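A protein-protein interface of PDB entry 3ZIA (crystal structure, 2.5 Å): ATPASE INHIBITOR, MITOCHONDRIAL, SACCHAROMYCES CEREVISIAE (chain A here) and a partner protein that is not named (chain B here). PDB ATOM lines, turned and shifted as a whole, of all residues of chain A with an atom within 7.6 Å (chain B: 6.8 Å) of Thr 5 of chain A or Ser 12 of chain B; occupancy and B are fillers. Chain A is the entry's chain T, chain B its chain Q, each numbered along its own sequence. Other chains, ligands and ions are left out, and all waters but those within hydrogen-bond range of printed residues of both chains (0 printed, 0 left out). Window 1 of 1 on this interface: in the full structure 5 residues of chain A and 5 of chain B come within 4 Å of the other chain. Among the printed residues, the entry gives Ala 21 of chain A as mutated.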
ATOM      1  N   SER A   1     -27.151   7.815  14.018  1.00  0.00           N
ATOM      2  CA  SER A   1     -28.512   8.388  13.800  1.00  0.00           C
ATOM      3  C   SER A   1     -28.846   9.521  14.781  1.00  0.00           C
ATOM      4  O   SER A   1     -29.327  10.576  14.368  1.00  0.00           O
ATOM      5  CB  SER A   1     -29.585   7.291  13.859  1.00  0.00           C
ATOM      6  OG  SER A   1     -30.889   7.846  13.792  1.00  0.00           O
ATOM      7  N   GLU A   2     -28.611   9.302  16.073  1.00  0.00           N
ATOM      8  CA  GLU A   2     -28.840  10.350  17.068  1.00  0.00           C
ATOM      9  C   GLU A   2     -27.681  11.330  17.048  1.00  0.00           C
ATOM     10  O   GLU A   2     -26.535  10.956  17.300  1.00  0.00           O
ATOM     11  CB  GLU A   2     -29.040   9.771  18.467  1.00  0.00           C
ATOM     12  CG  GLU A   2     -30.451   9.255  18.728  1.00  0.00           C
ATOM     13  CD  GLU A   2     -30.716   8.943  20.203  1.00  0.00           C
ATOM     14  OE1 GLU A   2     -29.918   9.358  21.078  1.00  0.00           O
ATOM     15  OE2 GLU A   2     -31.737   8.282  20.486  1.00  0.00           O
ATOM     16  N   GLY A   3     -27.990  12.580  16.722  1.00  0.00           N
ATOM     17  CA  GLY A   3     -26.975  13.620  16.600  1.00  0.00           C
ATOM     18  C   GLY A   3     -26.440  13.785  15.189  1.00  0.00           C
ATOM     19  O   GLY A   3     -25.564  14.615  14.938  1.00  0.00           O
ATOM     20  N   SER A   4     -26.982  12.994  14.270  1.00  0.00           N
ATOM     21  CA  SER A   4     -26.558  12.985  12.873  1.00  0.00           C
ATOM     22  C   SER A   4     -26.805  14.322  12.149  1.00  0.00           C
ATOM     23  O   SER A   4     -26.084  14.671  11.208  1.00  0.00           O
ATOM     24  CB  SER A   4     -27.248  11.834  12.141  1.00  0.00           C
ATOM     25  OG  SER A   4     -26.897  11.822  10.775  1.00  0.00           O
ATOM     26  N   THR A   5     -27.825  15.057  12.594  1.00  0.00           N
ATOM     27  CA  THR A   5     -28.120  16.390  12.076  1.00  0.00           C
ATOM     28  C   THR A   5     -27.424  17.477  12.898  1.00  0.00           C
ATOM     29  O   THR A   5     -26.827  18.399  12.338  1.00  0.00           O
ATOM     30  CB  THR A   5     -29.639  16.679  12.100  1.00  0.00           C
ATOM     31  OG1 THR A   5     -30.356  15.550  11.590  1.00  0.00           O
ATOM     32  CG2 THR A   5     -29.971  17.913  11.279  1.00  0.00           C
ATOM     33  N   GLY A   6     -27.503  17.358  14.224  1.00  0.00           N
ATOM     34  CA  GLY A   6     -27.155  18.457  15.120  1.00  0.00           C
ATOM     35  C   GLY A   6     -25.733  18.555  15.630  1.00  0.00           C
ATOM     36  O   GLY A   6     -25.195  19.656  15.751  1.00  0.00           O
ATOM     37  N   THR A   7     -25.117  17.419  15.933  1.00  0.00           N
ATOM     38  CA  THR A   7     -23.857  17.445  16.667  1.00  0.00           C
ATOM     39  C   THR A   7     -22.671  17.772  15.764  1.00  0.00           C
ATOM     40  O   THR A   7     -22.630  17.326  14.618  1.00  0.00           O
ATOM     41  CB  THR A   7     -23.618  16.153  17.499  1.00  0.00           C
ATOM     42  OG1 THR A   7     -22.931  15.172  16.722  1.00  0.00           O
ATOM     43  CG2 THR A   7     -24.924  15.585  17.971  1.00  0.00           C
ATOM     44  N   PRO A   8     -21.714  18.571  16.274  1.00  0.00           N
ATOM     45  CA  PRO A   8     -20.563  18.962  15.471  1.00  0.00           C
ATOM     46  C   PRO A   8     -19.535  17.846  15.296  1.00  0.00           C
ATOM     47  O   PRO A   8     -18.837  17.467  16.245  1.00  0.00           O
ATOM     48  CB  PRO A   8     -19.953  20.134  16.262  1.00  0.00           C
ATOM     49  CG  PRO A   8     -20.985  20.520  17.270  1.00  0.00           C
ATOM     50  CD  PRO A   8     -21.712  19.256  17.576  1.00  0.00           C
ATOM     51  N   ARG A   9     -19.472  17.320  14.079  1.00  0.00           N
ATOM     52  CA  ARG A   9     -18.341  16.528  13.621  1.00  0.00           C
ATOM     53  C   ARG A   9     -17.339  17.517  13.006  1.00  0.00           C
ATOM     54  O   ARG A   9     -17.526  18.735  13.106  1.00  0.00           O
ATOM     55  CB  ARG A   9     -18.811  15.486  12.607  1.00  0.00           C
ATOM     56  CG  ARG A   9     -19.460  16.096  11.389  1.00  0.00           C
ATOM     57  CD  ARG A   9     -20.822  15.517  11.128  1.00  0.00           C
ATOM     58  NE  ARG A   9     -21.508  16.345  10.146  1.00  0.00           N
ATOM     59  CZ  ARG A   9     -22.760  16.163   9.749  1.00  0.00           C
ATOM     60  NH1 ARG A   9     -23.484  15.172  10.250  1.00  0.00           N
ATOM     61  NH2 ARG A   9     -23.287  16.975   8.847  1.00  0.00           N
ATOM     62  N   ASP A  15     -22.742  20.790   7.982  1.00  0.00           N
ATOM     63  CA  ASP A  15     -23.992  21.243   7.386  1.00  0.00           C
ATOM     64  C   ASP A  15     -24.137  22.725   7.700  1.00  0.00           C
ATOM     65  O   ASP A  15     -23.353  23.290   8.472  1.00  0.00           O
ATOM     66  CB  ASP A  15     -25.189  20.521   8.014  1.00  0.00           C
ATOM     67  CG  ASP A  15     -25.314  19.085   7.576  1.00  0.00           C
ATOM     68  OD1 ASP A  15     -25.211  18.814   6.361  1.00  0.00           O
ATOM     69  OD2 ASP A  15     -25.551  18.226   8.459  1.00  0.00           O
ATOM     70  N   SER A  16     -25.150  23.351   7.112  1.00  0.00           N
ATOM     71  CA  SER A  16     -25.633  24.624   7.618  1.00  0.00           C
ATOM     72  C   SER A  16     -26.510  24.345   8.842  1.00  0.00           C
ATOM     73  O   SER A  16     -26.677  25.206   9.713  1.00  0.00           O
ATOM     74  CB  SER A  16     -26.408  25.385   6.538  1.00  0.00           C
ATOM     75  OG  SER A  16     -25.527  25.931   5.567  1.00  0.00           O
ATOM     76  N   PHE A  17     -27.048  23.126   8.903  1.00  0.00           N
ATOM     77  CA  PHE A  17     -27.878  22.667  10.017  1.00  0.00           C
ATOM     78  C   PHE A  17     -27.072  22.413  11.282  1.00  0.00           C
ATOM     79  O   PHE A  17     -27.557  22.661  12.380  1.00  0.00           O
ATOM     80  CB  PHE A  17     -28.659  21.416   9.621  1.00  0.00           C
ATOM     81  CG  PHE A  17     -29.677  21.659   8.549  1.00  0.00           C
ATOM     82  CD1 PHE A  17     -30.971  22.051   8.876  1.00  0.00           C
ATOM     83  CD2 PHE A  17     -29.341  21.505   7.208  1.00  0.00           C
ATOM     84  CE1 PHE A  17     -31.918  22.282   7.886  1.00  0.00           C
ATOM     85  CE2 PHE A  17     -30.284  21.737   6.204  1.00  0.00           C
ATOM     86  CZ  PHE A  17     -31.575  22.127   6.545  1.00  0.00           C
ATOM     87  N   VAL A  18     -25.851  21.907  11.126  1.00  0.00           N
ATOM     88  CA  VAL A  18     -24.911  21.806  12.238  1.00  0.00           C
ATOM     89  C   VAL A  18     -24.561  23.217  12.707  1.00  0.00           C
ATOM     90  O   VAL A  18     -24.586  23.505  13.905  1.00  0.00           O
ATOM     91  CB  VAL A  18     -23.617  21.054  11.835  1.00  0.00           C
ATOM     92  CG1 VAL A  18     -22.574  21.117  12.951  1.00  0.00           C
ATOM     93  CG2 VAL A  18     -23.920  19.616  11.478  1.00  0.00           C
ATOM     94  N   LYS A  19     -24.261  24.089  11.745  1.00  0.00           N
ATOM     95  CA  LYS A  19     -23.845  25.463  12.009  1.00  0.00           C
ATOM     96  C   LYS A  19     -24.891  26.258  12.793  1.00  0.00           C
ATOM     97  O   LYS A  19     -24.535  27.044  13.675  1.00  0.00           O
ATOM     98  CB  LYS A  19     -23.501  26.176  10.696  1.00  0.00           C
ATOM     99  CG  LYS A  19     -22.673  27.447  10.867  1.00  0.00           C
ATOM    100  CD  LYS A  19     -22.448  28.146   9.532  1.00  0.00           C
ATOM    101  CE  LYS A  19     -21.724  29.472   9.713  1.00  0.00           C
ATOM    102  NZ  LYS A  19     -21.725  30.259   8.449  1.00  0.00           N
ATOM    103  N   ALA A  21     -27.463  24.824  14.655  1.00  0.00           N
ATOM    104  CA  ALA A  21     -27.653  24.137  15.935  1.00  0.00           C
ATOM    105  C   ALA A  21     -26.697  24.681  16.985  1.00  0.00           C
ATOM    106  O   ALA A  21     -27.097  24.931  18.116  1.00  0.00           O
ATOM    107  CB  ALA A  21     -27.463  22.648  15.783  1.00  0.00           C
ATOM    108  N   GLU B   7     -23.171   9.199   2.990  1.00  0.00           N
ATOM    109  CA  GLU B   7     -23.832   8.520   4.104  1.00  0.00           C
ATOM    110  C   GLU B   7     -24.252   9.515   5.194  1.00  0.00           C
ATOM    111  O   GLU B   7     -25.415   9.542   5.589  1.00  0.00           O
ATOM    112  CB  GLU B   7     -22.932   7.417   4.682  1.00  0.00           C
ATOM    113  CG  GLU B   7     -23.671   6.430   5.590  1.00  0.00           C
ATOM    114  CD  GLU B   7     -22.737   5.505   6.375  1.00  0.00           C
ATOM    115  OE1 GLU B   7     -21.641   5.949   6.799  1.00  0.00           O
ATOM    116  OE2 GLU B   7     -23.113   4.327   6.577  1.00  0.00           O
ATOM    117  N   MET B   8     -23.301  10.332   5.656  1.00  0.00           N
ATOM    118  CA  MET B   8     -23.548  11.355   6.681  1.00  0.00           C
ATOM    119  C   MET B   8     -24.658  12.310   6.274  1.00  0.00           C
ATOM    120  O   MET B   8     -25.633  12.495   7.014  1.00  0.00           O
ATOM    121  CB  MET B   8     -22.279  12.153   6.976  1.00  0.00           C
ATOM    122  CG  MET B   8     -21.267  11.422   7.840  1.00  0.00           C
ATOM    123  SD  MET B   8     -19.851  12.485   8.175  1.00  0.00           S
ATOM    124  CE  MET B   8     -18.907  11.439   9.292  1.00  0.00           C
ATOM    125  N   ARG B   9     -24.495  12.903   5.092  1.00  0.00           N
ATOM    126  CA  ARG B   9     -25.499  13.755   4.479  1.00  0.00           C
ATOM    127  C   ARG B   9     -26.863  13.062   4.469  1.00  0.00           C
ATOM    128  O   ARG B   9     -27.863  13.659   4.847  1.00  0.00           O
ATOM    129  CB  ARG B   9     -25.055  14.143   3.060  1.00  0.00           C
ATOM    130  CG  ARG B   9     -25.673  15.422   2.498  1.00  0.00           C
ATOM    131  CD  ARG B   9     -25.060  16.692   3.101  1.00  0.00           C
ATOM    132  NE  ARG B   9     -25.942  17.863   2.957  1.00  0.00           N
ATOM    133  CZ  ARG B   9     -26.858  18.260   3.849  1.00  0.00           C
ATOM    134  NH1 ARG B   9     -27.054  17.596   4.989  1.00  0.00           N
ATOM    135  NH2 ARG B   9     -27.590  19.338   3.603  1.00  0.00           N
ATOM    136  N   LEU B  10     -26.888  11.794   4.078  1.00  0.00           N
ATOM    137  CA  LEU B  10     -28.132  11.036   3.969  1.00  0.00           C
ATOM    138  C   LEU B  10     -28.838  10.804   5.316  1.00  0.00           C
ATOM    139  O   LEU B  10     -30.041  11.004   5.429  1.00  0.00           O
ATOM    140  CB  LEU B  10     -27.865   9.709   3.240  1.00  0.00           C
ATOM    141  CG  LEU B  10     -28.960   8.875   2.577  1.00  0.00           C
ATOM    142  CD1 LEU B  10     -29.914   9.719   1.759  1.00  0.00           C
ATOM    143  CD2 LEU B  10     -28.314   7.829   1.697  1.00  0.00           C
ATOM    144  N   LYS B  11     -28.087  10.383   6.333  1.00  0.00           N
ATOM    145  CA  LYS B  11     -28.633  10.195   7.686  1.00  0.00           C
ATOM    146  C   LYS B  11     -29.089  11.513   8.313  1.00  0.00           C
ATOM    147  O   LYS B  11     -30.045  11.520   9.090  1.00  0.00           O
ATOM    148  CB  LYS B  11     -27.615   9.512   8.611  1.00  0.00           C
ATOM    149  CG  LYS B  11     -27.528   7.983   8.469  1.00  0.00           C
ATOM    150  CD  LYS B  11     -26.125   7.453   8.845  1.00  0.00           C
ATOM    151  CE  LYS B  11     -25.872   7.493  10.347  1.00  0.00           C
ATOM    152  NZ  LYS B  11     -24.441   7.231  10.672  1.00  0.00           N
ATOM    153  N   SER B  12     -28.406  12.609   7.982  1.00  0.00           N
ATOM    154  CA  SER B  12     -28.759  13.929   8.504  1.00  0.00           C
ATOM    155  C   SER B  12     -30.112  14.406   7.983  1.00  0.00           C
ATOM    156  O   SER B  12     -30.955  14.869   8.756  1.00  0.00           O
ATOM    157  CB  SER B  12     -27.678  14.959   8.178  1.00  0.00           C
ATOM    158  OG  SER B  12     -28.037  16.249   8.648  1.00  0.00           O
ATOM    159  N   ILE B  13     -30.313  14.281   6.674  1.00  0.00           N
ATOM    160  CA  ILE B  13     -31.562  14.671   6.027  1.00  0.00           C
ATOM    161  C   ILE B  13     -32.700  13.717   6.385  1.00  0.00           C
ATOM    162  O   ILE B  13     -33.869  14.114   6.391  1.00  0.00           O
ATOM    163  CB  ILE B  13     -31.393  14.762   4.493  1.00  0.00           C
ATOM    164  CG1 ILE B  13     -30.310  15.780   4.134  1.00  0.00           C
ATOM    165  CG2 ILE B  13     -32.694  15.156   3.807  1.00  0.00           C
ATOM    166  CD1 ILE B  13     -29.796  15.644   2.712  1.00  0.00           C
ATOM    167  N   LYS B  14     -32.364  12.463   6.687  1.00  0.00           N
ATOM    168  CA  LYS B  14     -33.369  11.471   7.079  1.00  0.00           C
ATOM    169  C   LYS B  14     -34.021  11.818   8.418  1.00  0.00           C
ATOM    170  O   LYS B  14     -35.217  11.565   8.616  1.00  0.00           O
ATOM    171  CB  LYS B  14     -32.782  10.056   7.103  1.00  0.00           C
ATOM    172  CG  LYS B  14     -32.825   9.345   5.755  1.00  0.00           C
ATOM    173  CD  LYS B  14     -32.391   7.897   5.874  1.00  0.00           C
ATOM    174  CE  LYS B  14     -32.677   7.137   4.588  1.00  0.00           C
ATOM    175  NZ  LYS B  14     -32.368   5.689   4.723  1.00  0.00           N
ATOM    176  N   ASN B  15     -33.219  12.390   9.322  1.00  0.00           N
ATOM    177  CA  ASN B  15     -33.703  12.927  10.597  1.00  0.00           C
ATOM    178  C   ASN B  15     -34.544  14.167  10.377  1.00  0.00           C
ATOM    179  O   ASN B  15     -35.636  14.288  10.931  1.00  0.00           O
ATOM    180  CB  ASN B  15     -32.539  13.266  11.534  1.00  0.00           C
ATOM    181  CG  ASN B  15     -32.011  12.057  12.278  1.00  0.00           C
ATOM    182  OD1 ASN B  15     -32.552  10.954  12.176  1.00  0.00           O
ATOM    183  ND2 ASN B  15     -30.945  12.262  13.038  1.00  0.00           N
ATOM    184  N   ILE B  16     -34.030  15.082   9.562  1.00  0.00           N
ATOM    185  CA  ILE B  16     -34.768  16.290   9.211  1.00  0.00           C
ATOM    186  C   ILE B  16     -36.169  15.943   8.720  1.00  0.00           C
ATOM    187  O   ILE B  16     -37.147  16.498   9.202  1.00  0.00           O
ATOM    188  CB  ILE B  16     -34.019  17.153   8.185  1.00  0.00           C
ATOM    189  CG1 ILE B  16     -32.746  17.719   8.824  1.00  0.00           C
ATOM    190  CG2 ILE B  16     -34.920  18.273   7.685  1.00  0.00           C
ATOM    191  CD1 ILE B  16     -31.876  18.526   7.901  1.00  0.00           C
ATOM    192  N   GLU B  17     -36.266  14.995   7.796  1.00  0.00           N
ATOM    193  CA  GLU B  17     -37.563  14.569   7.301  1.00  0.00           C
ATOM    194  C   GLU B  17     -38.461  14.103   8.442  1.00  0.00           C
ATOM    195  O   GLU B  17     -39.643  14.439   8.487  1.00  0.00           O
ATOM    196  CB  GLU B  17     -37.418  13.465   6.259  1.00  0.00           C
ATOM    197  CG  GLU B  17     -38.706  13.161   5.506  1.00  0.00           C
ATOM    198  CD  GLU B  17     -38.771  11.732   5.000  1.00  0.00           C
ATOM    199  OE1 GLU B  17     -37.988  10.885   5.487  1.00  0.00           O
ATOM    200  OE2 GLU B  17     -39.614  11.454   4.116  1.00  0.00           O
ATOM    201  N   ILE B  19     -38.195  14.798  11.797  1.00  0.00           N
ATOM    202  CA  ILE B  19     -38.480  15.882  12.745  1.00  0.00           C
ATOM    203  C   ILE B  19     -39.571  16.817  12.200  1.00  0.00           C
ATOM    204  O   ILE B  19     -40.563  17.100  12.887  1.00  0.00           O
ATOM    205  CB  ILE B  19     -37.195  16.730  13.104  1.00  0.00           C
ATOM    206  CG1 ILE B  19     -35.967  15.857  13.440  1.00  0.00           C
ATOM    207  CG2 ILE B  19     -37.493  17.738  14.211  1.00  0.00           C
ATOM    208  CD1 ILE B  19     -36.080  14.961  14.669  1.00  0.00           C
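Thr 5 of chain A touches just these residues of chain B: Ser 12, Asn 15 and Ile 16. Ser 12 of chain B touches just these residues of chain A: Ser 4, Thr 5 and Asp 15. Of the printed residues of chain A, Arg 9 of chain B touches Asp 15 (2.6 Å). Of the printed residues of chain A, Lys 11 of chain B touches Ser 1 and Ser 4. Of the printed residues of chain A, Asn 15 of chain B touches Ser 1 (2.7 Å), Ser 4 (3.8 Å) and Thr 5 (3.2 Å). Of the printed residues of chain B, Asp 15 of chain A touches Arg 9 (2.6 Å) and Ser 12 (3.2 Å). The nearest residue of chain B that does not touch Thr 5 of chain A is Lys 11 of chain B (4.8 Å). The nearest residue of chain A that does not touch Ser 12 of chain B is Arg 9 of chain A (4.7 Å).
Printed residues of chain A that touch a printed residue of chain B: Ser 1, Ser 4, Thr 5, Asp 15 and Phe 17. Hydrophobic or aromatic side chains of chain A that line the printed part of chain B: Phe 17. Of the 12 printed residues of chain B, 5 touch a printed residue of chain A. Hydrophobic or aromatic side chains of chain B that line the printed part of chain A: Ile 16. Among the printed residues, 11 pairs touch across the chains.
The guanidinium group (NH1) of Arg 9 of chain B lies within salt-bridge range of the side-chain carboxylate (OD1) of Asp 15 of chain A (2.6 Å). The side-chain hydroxyl (OG) of Ser 4 of chain A is in hydrogen-bond range of the backbone NH (N) of Ser 12 of chain B, at 3.3 Å. The side-chain hydroxyl (OG1) of Thr 5 of chain A is in hydrogen-bond range of the backbone carbonyl oxygen (O) of Ser 12 of chain B (3.0 Å). OG of Ser 12 of chain B sits at hydrogen-bond distance from OD2 of Asp 15 of chain A, at 3.2 Å. The side-chain amide nitrogen (ND2) of Asn 15 of chain B lies within hydrogen-bond range of the backbone carbonyl oxygen (O) of Ser 1 of chain A, 2.7 Å away.
O of Ser 4 of chain A is in hydrogen-bond range of NH1 of Arg 9 of chain A (2.8 Å). The guanidinium group (NH2) of Arg 9 of chain A lies within salt-bridge range of the side-chain carboxylate (OD2) of Asp 15 of chain A (2.6 Å).
N of Ser 1 of chain A touches CE of Lys 11 of chain B, at 3.9 Å. Lys 11 of chain B touches Ser 4 of chain A (CB to OG, 3.2 Å). Asn 15 of chain B touches Ser 4 of chain A (ND2 to CB, 3.8 Å). OG1 of Thr 5 of chain A touches CB of Asn 15 of chain B, 3.2 Å away. CG1 of Ile 16 of chain B touches CG2 of Thr 5 of chain A, at 3.7 Å. Phe 17 of chain A touches Ile 16 of chain B.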
